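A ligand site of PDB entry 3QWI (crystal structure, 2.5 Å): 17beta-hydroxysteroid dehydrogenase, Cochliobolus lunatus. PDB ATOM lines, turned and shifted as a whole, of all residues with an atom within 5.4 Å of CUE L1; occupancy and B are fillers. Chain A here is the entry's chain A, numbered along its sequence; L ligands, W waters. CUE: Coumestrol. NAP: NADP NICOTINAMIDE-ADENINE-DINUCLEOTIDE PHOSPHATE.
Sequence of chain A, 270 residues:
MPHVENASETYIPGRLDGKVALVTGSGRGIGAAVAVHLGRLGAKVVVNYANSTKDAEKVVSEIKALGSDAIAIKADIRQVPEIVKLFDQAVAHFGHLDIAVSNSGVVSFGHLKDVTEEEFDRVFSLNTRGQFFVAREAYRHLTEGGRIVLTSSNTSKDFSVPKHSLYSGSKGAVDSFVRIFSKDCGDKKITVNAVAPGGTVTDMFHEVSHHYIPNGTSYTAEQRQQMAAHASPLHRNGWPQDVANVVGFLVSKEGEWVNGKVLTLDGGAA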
ATOM      1  N   VAL A 107       5.341 -11.899   0.243  1.00  0.00           N
ATOM      2  CA  VAL A 107       4.516 -12.668  -0.688  1.00  0.00           C
ATOM      3  C   VAL A 107       5.146 -14.042  -0.948  1.00  0.00           C
ATOM      4  O   VAL A 107       6.321 -14.257  -0.652  1.00  0.00           O
ATOM      5  CB  VAL A 107       4.303 -11.894  -2.010  1.00  0.00           C
ATOM      6  CG1 VAL A 107       5.561 -11.933  -2.903  1.00  0.00           C
ATOM      7  CG2 VAL A 107       3.076 -12.413  -2.750  1.00  0.00           C
ATOM      8  N   ASN A 154      -6.451  -8.553  -2.121  1.00  0.00           N
ATOM      9  CA  ASN A 154      -7.571  -8.946  -2.988  1.00  0.00           C
ATOM     10  C   ASN A 154      -7.610 -10.468  -3.187  1.00  0.00           C
ATOM     11  O   ASN A 154      -8.652 -11.047  -3.531  1.00  0.00           O
ATOM     12  CB  ASN A 154      -7.548  -8.216  -4.327  1.00  0.00           C
ATOM     13  CG  ASN A 154      -6.455  -8.706  -5.249  1.00  0.00           C
ATOM     14  OD1 ASN A 154      -5.355  -9.051  -4.832  1.00  0.00           O
ATOM     15  ND2 ASN A 154      -6.749  -8.729  -6.539  1.00  0.00           N
ATOM     16  N   THR A 155      -6.459 -11.108  -2.970  1.00  0.00           N
ATOM     17  CA  THR A 155      -6.334 -12.560  -3.104  1.00  0.00           C
ATOM     18  C   THR A 155      -6.846 -13.301  -1.868  1.00  0.00           C
ATOM     19  O   THR A 155      -6.946 -14.522  -1.861  1.00  0.00           O
ATOM     20  CB  THR A 155      -4.879 -12.984  -3.396  1.00  0.00           C
ATOM     21  OG1 THR A 155      -4.009 -12.496  -2.353  1.00  0.00           O
ATOM     22  CG2 THR A 155      -4.421 -12.432  -4.731  1.00  0.00           C
ATOM     23  N   PHE A 159     -10.039 -12.581  -5.262  1.00  0.00           N
ATOM     24  CA  PHE A 159      -9.277 -12.982  -6.443  1.00  0.00           C
ATOM     25  C   PHE A 159      -8.622 -14.343  -6.192  1.00  0.00           C
ATOM     26  O   PHE A 159      -7.918 -14.517  -5.208  1.00  0.00           O
ATOM     27  CB  PHE A 159      -8.245 -11.898  -6.767  1.00  0.00           C
ATOM     28  CG  PHE A 159      -7.531 -12.074  -8.097  1.00  0.00           C
ATOM     29  CD1 PHE A 159      -8.212 -12.553  -9.218  1.00  0.00           C
ATOM     30  CD2 PHE A 159      -6.192 -11.723  -8.228  1.00  0.00           C
ATOM     31  CE1 PHE A 159      -7.553 -12.698 -10.436  1.00  0.00           C
ATOM     32  CE2 PHE A 159      -5.535 -11.858  -9.444  1.00  0.00           C
ATOM     33  CZ  PHE A 159      -6.213 -12.351 -10.545  1.00  0.00           C
ATOM     34  N   TYR A 167      -0.214 -17.539   0.921  1.00  0.00           N
ATOM     35  CA  TYR A 167      -0.334 -16.088   1.063  1.00  0.00           C
ATOM     36  C   TYR A 167      -1.790 -15.659   1.219  1.00  0.00           C
ATOM     37  O   TYR A 167      -2.106 -14.830   2.061  1.00  0.00           O
ATOM     38  CB  TYR A 167       0.312 -15.380  -0.133  1.00  0.00           C
ATOM     39  CG  TYR A 167       0.186 -13.877  -0.109  1.00  0.00           C
ATOM     40  CD1 TYR A 167       1.071 -13.092   0.632  1.00  0.00           C
ATOM     41  CD2 TYR A 167      -0.807 -13.234  -0.854  1.00  0.00           C
ATOM     42  CE1 TYR A 167       0.965 -11.695   0.636  1.00  0.00           C
ATOM     43  CE2 TYR A 167      -0.920 -11.849  -0.847  1.00  0.00           C
ATOM     44  CZ  TYR A 167      -0.040 -11.086  -0.105  1.00  0.00           C
ATOM     45  OH  TYR A 167      -0.167  -9.722  -0.115  1.00  0.00           O
ATOM     46  N   GLY A 198      -5.164  -4.669  -4.553  1.00  0.00           N
ATOM     47  CA  GLY A 198      -4.879  -5.556  -5.668  1.00  0.00           C
ATOM     48  C   GLY A 198      -3.460  -5.285  -6.120  1.00  0.00           C
ATOM     49  O   GLY A 198      -2.647  -4.745  -5.361  1.00  0.00           O
ATOM     50  N   GLY A 199      -3.155  -5.658  -7.362  1.00  0.00           N
ATOM     51  CA  GLY A 199      -1.835  -5.397  -7.921  1.00  0.00           C
ATOM     52  C   GLY A 199      -1.429  -3.939  -7.833  1.00  0.00           C
ATOM     53  O   GLY A 199      -1.955  -3.094  -8.572  1.00  0.00           O
ATOM     54  N   THR A 200      -0.486  -3.648  -6.938  1.00  0.00           N
ATOM     55  CA  THR A 200       0.010  -2.306  -6.692  1.00  0.00           C
ATOM     56  C   THR A 200       1.501  -2.272  -7.021  1.00  0.00           C
ATOM     57  O   THR A 200       2.264  -3.122  -6.569  1.00  0.00           O
ATOM     58  CB  THR A 200      -0.226  -1.912  -5.212  1.00  0.00           C
ATOM     59  OG1 THR A 200      -1.574  -2.216  -4.846  1.00  0.00           O
ATOM     60  CG2 THR A 200       0.016  -0.431  -4.978  1.00  0.00           C
ATOM     61  N   MET A 204       7.208  -5.766  -4.561  1.00  0.00           N
ATOM     62  CA  MET A 204       6.412  -6.986  -4.487  1.00  0.00           C
ATOM     63  C   MET A 204       5.766  -7.316  -5.819  1.00  0.00           C
ATOM     64  O   MET A 204       5.701  -8.486  -6.213  1.00  0.00           O
ATOM     65  CB  MET A 204       5.340  -6.894  -3.405  1.00  0.00           C
ATOM     66  CG  MET A 204       4.552  -8.182  -3.240  1.00  0.00           C
ATOM     67  SD  MET A 204       3.547  -8.224  -1.761  1.00  0.00           S
ATOM     68  CE  MET A 204       4.814  -8.415  -0.499  1.00  0.00           C
ATOM     69  N   PHE A 205       5.268  -6.282  -6.489  1.00  0.00           N
ATOM     70  CA  PHE A 205       4.636  -6.439  -7.790  1.00  0.00           C
ATOM     71  C   PHE A 205       5.597  -7.121  -8.761  1.00  0.00           C
ATOM     72  O   PHE A 205       5.255  -8.130  -9.357  1.00  0.00           O
ATOM     73  CB  PHE A 205       4.128  -5.090  -8.325  1.00  0.00           C
ATOM     74  CG  PHE A 205       3.263  -5.220  -9.568  1.00  0.00           C
ATOM     75  CD1 PHE A 205       3.840  -5.247 -10.835  1.00  0.00           C
ATOM     76  CD2 PHE A 205       1.873  -5.308  -9.457  1.00  0.00           C
ATOM     77  CE1 PHE A 205       3.046  -5.371 -11.979  1.00  0.00           C
ATOM     78  CE2 PHE A 205       1.070  -5.424 -10.594  1.00  0.00           C
ATOM     79  CZ  PHE A 205       1.661  -5.459 -11.859  1.00  0.00           C
ATOM     80  N   VAL A 208       6.362 -10.975  -8.120  1.00  0.00           N
ATOM     81  CA  VAL A 208       5.438 -12.053  -8.444  1.00  0.00           C
ATOM     82  C   VAL A 208       4.400 -11.826  -9.553  1.00  0.00           C
ATOM     83  O   VAL A 208       3.486 -12.646  -9.690  1.00  0.00           O
ATOM     84  CB  VAL A 208       4.729 -12.601  -7.167  1.00  0.00           C
ATOM     85  CG1 VAL A 208       5.719 -13.372  -6.295  1.00  0.00           C
ATOM     86  CG2 VAL A 208       4.041 -11.488  -6.397  1.00  0.00           C
ATOM     87  N   SER A 209       4.528 -10.755 -10.338  1.00  0.00           N
ATOM     88  CA  SER A 209       3.527 -10.432 -11.368  1.00  0.00           C
ATOM     89  C   SER A 209       3.374 -11.551 -12.404  1.00  0.00           C
ATOM     90  O   SER A 209       2.276 -11.770 -12.904  1.00  0.00           O
ATOM     91  CB  SER A 209       3.802  -9.084 -12.049  1.00  0.00           C
ATOM     92  OG  SER A 209       5.013  -9.066 -12.799  1.00  0.00           O
ATOM     93  N   TYR A 212       0.731 -14.141 -11.583  1.00  0.00           N
ATOM     94  CA  TYR A 212      -0.663 -13.709 -11.710  1.00  0.00           C
ATOM     95  C   TYR A 212      -1.188 -13.735 -13.160  1.00  0.00           C
ATOM     96  O   TYR A 212      -2.354 -13.401 -13.418  1.00  0.00           O
ATOM     97  CB  TYR A 212      -0.812 -12.296 -11.169  1.00  0.00           C
ATOM     98  CG  TYR A 212      -0.800 -12.201  -9.666  1.00  0.00           C
ATOM     99  CD1 TYR A 212       0.395 -12.085  -8.965  1.00  0.00           C
ATOM    100  CD2 TYR A 212      -1.996 -12.200  -8.946  1.00  0.00           C
ATOM    101  CE1 TYR A 212       0.402 -11.993  -7.562  1.00  0.00           C
ATOM    102  CE2 TYR A 212      -2.000 -12.097  -7.559  1.00  0.00           C
ATOM    103  CZ  TYR A 212      -0.798 -11.997  -6.874  1.00  0.00           C
ATOM    104  OH  TYR A 212      -0.815 -11.895  -5.492  1.00  0.00           O
ATOM    105  N   ILE A 213      -0.312 -14.111 -14.082  1.00  0.00           N
ATOM    106  CA  ILE A 213      -0.617 -14.100 -15.510  1.00  0.00           C
ATOM    107  C   ILE A 213      -0.297 -15.454 -16.137  1.00  0.00           C
ATOM    108  O   ILE A 213       0.786 -16.004 -15.911  1.00  0.00           O
ATOM    109  CB  ILE A 213       0.161 -12.959 -16.229  1.00  0.00           C
ATOM    110  CG1 ILE A 213      -0.398 -11.591 -15.813  1.00  0.00           C
ATOM    111  CG2 ILE A 213       0.124 -13.137 -17.760  1.00  0.00           C
ATOM    112  CD1 ILE A 213       0.595 -10.468 -15.829  1.00  0.00           C
ATOM    113  N   ARG A 224       3.765  -7.078 -18.412  1.00  0.00           N
ATOM    114  CA  ARG A 224       3.023  -7.568 -17.260  1.00  0.00           C
ATOM    115  C   ARG A 224       2.369  -6.423 -16.517  1.00  0.00           C
ATOM    116  O   ARG A 224       1.233  -6.547 -16.067  1.00  0.00           O
ATOM    117  CB  ARG A 224       3.924  -8.377 -16.332  1.00  0.00           C
ATOM    118  CG  ARG A 224       3.812  -9.869 -16.546  1.00  0.00           C
ATOM    119  CD  ARG A 224       5.154 -10.559 -16.641  1.00  0.00           C
ATOM    120  NE  ARG A 224       5.996 -10.359 -15.471  1.00  0.00           N
ATOM    121  CZ  ARG A 224       7.327 -10.369 -15.502  1.00  0.00           C
ATOM    122  NH1 ARG A 224       7.981 -10.561 -16.642  1.00  0.00           N
ATOM    123  NH2 ARG A 224       8.023 -10.187 -14.381  1.00  0.00           N
ATOM    124  N   MET A 227      -0.625  -5.370 -18.612  1.00  0.00           N
ATOM    125  CA  MET A 227      -1.709  -6.349 -18.513  1.00  0.00           C
ATOM    126  C   MET A 227      -2.430  -6.208 -17.170  1.00  0.00           C
ATOM    127  O   MET A 227      -3.647  -6.392 -17.092  1.00  0.00           O
ATOM    128  CB  MET A 227      -1.182  -7.779 -18.688  1.00  0.00           C
ATOM    129  CG  MET A 227      -0.855  -8.151 -20.135  1.00  0.00           C
ATOM    130  SD  MET A 227      -0.148  -9.808 -20.244  1.00  0.00           S
ATOM    131  CE  MET A 227      -1.562 -10.823 -19.789  1.00  0.00           C
ATOM    132  N   ALA A 228      -1.657  -5.905 -16.125  1.00  0.00           N
ATOM    133  CA  ALA A 228      -2.211  -5.688 -14.798  1.00  0.00           C
ATOM    134  C   ALA A 228      -3.081  -4.438 -14.783  1.00  0.00           C
ATOM    135  O   ALA A 228      -4.083  -4.380 -14.060  1.00  0.00           O
ATOM    136  CB  ALA A 228      -1.108  -5.566 -13.774  1.00  0.00           C
ATOM    137  N   ALA A 231      -6.564  -5.088 -15.839  1.00  0.00           N
ATOM    138  CA  ALA A 231      -7.405  -5.783 -14.856  1.00  0.00           C
ATOM    139  C   ALA A 231      -8.530  -4.839 -14.401  1.00  0.00           C
ATOM    140  O   ALA A 231      -9.713  -5.180 -14.502  1.00  0.00           O
ATOM    141  CB  ALA A 231      -6.591  -6.267 -13.649  1.00  0.00           C
HETATM  142  OAA CUE L   1      -4.359  -8.769  -8.664  1.00  0.00           O
HETATM  143  OAB CUE L   1       1.217  -8.708  -4.479  1.00  0.00           O
HETATM  144  OAC CUE L   1      -2.588  -9.284 -15.207  1.00  0.00           O
HETATM  145  CAD CUE L   1       1.541  -8.688  -6.869  1.00  0.00           C
HETATM  146  CAE CUE L   1      -3.835  -9.195 -13.178  1.00  0.00           C
HETATM  147  CAF CUE L   1       0.999  -8.718  -8.151  1.00  0.00           C
HETATM  148  CAG CUE L   1      -3.841  -9.105 -11.779  1.00  0.00           C
HETATM  149  CAH CUE L   1      -0.675  -8.799  -5.918  1.00  0.00           C
HETATM  150  CAI CUE L   1      -1.413  -9.103 -13.148  1.00  0.00           C
HETATM  151  OAJ CUE L   1      -2.597  -8.904  -7.310  1.00  0.00           O
HETATM  152  OAK CUE L   1      -0.409  -8.906 -10.848  1.00  0.00           O
HETATM  153  CAL CUE L   1       0.710  -8.732  -5.756  1.00  0.00           C
HETATM  154  CAM CUE L   1      -2.618  -9.190 -13.853  1.00  0.00           C
HETATM  155  CAN CUE L   1      -3.135  -8.866  -8.566  1.00  0.00           C
HETATM  156  CAO CUE L   1      -1.227  -8.831  -7.196  1.00  0.00           C
HETATM  157  CAP CUE L   1      -1.425  -9.002 -11.757  1.00  0.00           C
HETATM  158  CAQ CUE L   1      -0.395  -8.764  -8.318  1.00  0.00           C
HETATM  159  CAR CUE L   1      -2.638  -9.008 -11.073  1.00  0.00           C
HETATM  160  CAS CUE L   1      -0.958  -8.831  -9.592  1.00  0.00           C
HETATM  161  CAT CUE L   1      -2.341  -8.906  -9.710  1.00  0.00           C
HETATM  162  PA  NAP L   2       7.240  -4.534  -0.640  1.00  0.00           P
HETATM  163  O1A NAP L   2       7.963  -5.800  -0.884  1.00  0.00           O
HETATM  164  O2A NAP L   2       7.392  -3.425  -1.606  1.00  0.00           O
HETATM  165  O5B NAP L   2       7.586  -3.994   0.813  1.00  0.00           O
HETATM  166  C5B NAP L   2       7.486  -4.847   1.955  1.00  0.00           C
HETATM  167  C4B NAP L   2       7.602  -4.031   3.247  1.00  0.00           C
HETATM  168  O4B NAP L   2       7.496  -4.946   4.387  1.00  0.00           O
HETATM  169  C3B NAP L   2       8.978  -3.345   3.353  1.00  0.00           C
HETATM  170  O3B NAP L   2       8.821  -2.030   3.913  1.00  0.00           O
HETATM  171  C2B NAP L   2       9.744  -4.249   4.323  1.00  0.00           C
HETATM  172  O2B NAP L   2      10.717  -3.520   5.069  1.00  0.00           O
HETATM  173  C1B NAP L   2       8.625  -4.679   5.272  1.00  0.00           C
HETATM  174  N9A NAP L   2       9.116  -5.865   6.024  1.00  0.00           N
HETATM  175  C8A NAP L   2       9.491  -7.053   5.506  1.00  0.00           C
HETATM  176  N7A NAP L   2       9.891  -7.855   6.498  1.00  0.00           N
HETATM  177  C5A NAP L   2       9.765  -7.182   7.646  1.00  0.00           C
HETATM  178  C6A NAP L   2      10.007  -7.486   8.970  1.00  0.00           C
HETATM  179  N6A NAP L   2      10.481  -8.682   9.320  1.00  0.00           N
HETATM  180  N1A NAP L   2       9.771  -6.548   9.915  1.00  0.00           N
HETATM  181  C2A NAP L   2       9.319  -5.342   9.588  1.00  0.00           C
HETATM  182  N3A NAP L   2       9.077  -5.017   8.323  1.00  0.00           N
HETATM  183  C4A NAP L   2       9.282  -5.913   7.341  1.00  0.00           C
HETATM  184  O3  NAP L   2       5.677  -4.930  -0.496  1.00  0.00           O
HETATM  185  PN  NAP L   2       4.466  -3.850  -0.586  1.00  0.00           P
HETATM  186  O1N NAP L   2       4.859  -2.561   0.063  1.00  0.00           O
HETATM  187  O2N NAP L   2       3.963  -3.852  -1.978  1.00  0.00           O
HETATM  188  O5D NAP L   2       3.405  -4.560   0.366  1.00  0.00           O
HETATM  189  C5D NAP L   2       3.035  -4.015   1.622  1.00  0.00           C
HETATM  190  C4D NAP L   2       1.797  -4.779   2.130  1.00  0.00           C
HETATM  191  O4D NAP L   2       0.788  -4.749   1.103  1.00  0.00           O
HETATM  192  C3D NAP L   2       2.121  -6.244   2.378  1.00  0.00           C
HETATM  193  O3D NAP L   2       1.417  -6.646   3.540  1.00  0.00           O
HETATM  194  C2D NAP L   2       1.540  -6.933   1.152  1.00  0.00           C
HETATM  195  O2D NAP L   2       1.174  -8.285   1.427  1.00  0.00           O
HETATM  196  C1D NAP L   2       0.305  -6.087   0.907  1.00  0.00           C
HETATM  197  N1N NAP L   2      -0.148  -6.211  -0.499  1.00  0.00           N
HETATM  198  C2N NAP L   2       0.645  -5.766  -1.580  1.00  0.00           C
HETATM  199  C3N NAP L   2       0.170  -5.913  -2.885  1.00  0.00           C
HETATM  200  C7N NAP L   2       0.959  -5.432  -4.109  1.00  0.00           C
HETATM  201  O7N NAP L   2       0.417  -5.562  -5.354  1.00  0.00           O
HETATM  202  N7N NAP L   2       2.150  -4.870  -3.914  1.00  0.00           N
HETATM  203  C4N NAP L   2      -1.076  -6.501  -3.109  1.00  0.00           C
HETATM  204  C5N NAP L   2      -1.853  -6.950  -2.048  1.00  0.00           C
HETATM  205  C6N NAP L   2      -1.400  -6.807  -0.743  1.00  0.00           C
HETATM  206  P2B NAP L   2      12.298  -3.837   4.992  1.00  0.00           P
HETATM  207  O1X NAP L   2      13.055  -2.926   5.869  1.00  0.00           O
HETATM  208  O2X NAP L   2      12.727  -3.689   3.466  1.00  0.00           O
HETATM  209  O3X NAP L   2      12.528  -5.382   5.352  1.00  0.00           O
HETATM  210  O   HOH W   1      -5.706  -5.976  -9.310  1.00  0.00           O
HETATM  211  O   HOH W   2      -7.161  -8.318 -10.105  1.00  0.00           O
HETATM  212  O   HOH W   3      -2.908  -9.656  -3.646  1.00  0.00           O
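Water W1 lies within hydrogen-bond range of OAA of CUE L1 (3.2 Å) and N of Gly 199 (3.2 Å).
Water W3 lies within hydrogen-bond range of the side-chain amide oxygen (OD1) of Asn 154 (2.8 Å) and the side-chain hydroxyl (OG1) of Thr 155 (3.3 Å).
The side-chain amide nitrogen (ND2) of Asn 154 lies within hydrogen-bond range of an oxygen (OAA) of CUE L1 (3.2 Å).
The side-chain hydroxyl (OH) of Tyr 167 lies within hydrogen-bond range of an oxygen (O2D) of NAP L2, at 2.5 Å.
The backbone NH of Gly 199 lies within hydrogen-bond range of an oxygen (OAJ) of CUE L1.
The backbone carbonyl oxygen of Thr 200 is in hydrogen-bond range of a nitrogen (N7N) of NAP L2 (3.2 Å).
An oxygen (O7N) of NAP L2 is in hydrogen-bond range of the backbone NH of Thr 200, 2.6 Å away.
OAB of CUE L1 lies close to SD of Met 204 (3.6 Å).
O7N of NAP L2 lies close to OAB of CUE L1.
O of Gly 198 is in hydrogen-bond range of OG1 of Thr 200 (2.8 Å).
The backbone carbonyl oxygen of Asn 154 sits at hydrogen-bond distance from the backbone NH of Phe 159 (2.7 Å).
CE2 of Phe 159 touches OAA of CUE L1, at 3.4 Å.
Gly 198 touches CUE L1 (C to OAJ, 3.9 Å).
Phe 205 touches CUE L1 (CD2 to CAF, 3.8 Å).
Val 208 touches CUE L1.
Tyr 212 touches CUE L1 (OH to CAH, 3.1 Å).
CG1 of Ile 213 touches OAC of CUE L1, at 3.2 Å.
Met 227 touches CUE L1.
Ala 228 touches CUE L1.
11 residues have an atom within 4 Å of CUE L1: Asn 154, Phe 159, Gly 198, Gly 199, Met 204, Phe 205, Val 208, Tyr 212, Ile 213, Met 227 and Ala 228.
The nearest printed residue that does not touch CUE L1 is Ala 231 (4.05 Å).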
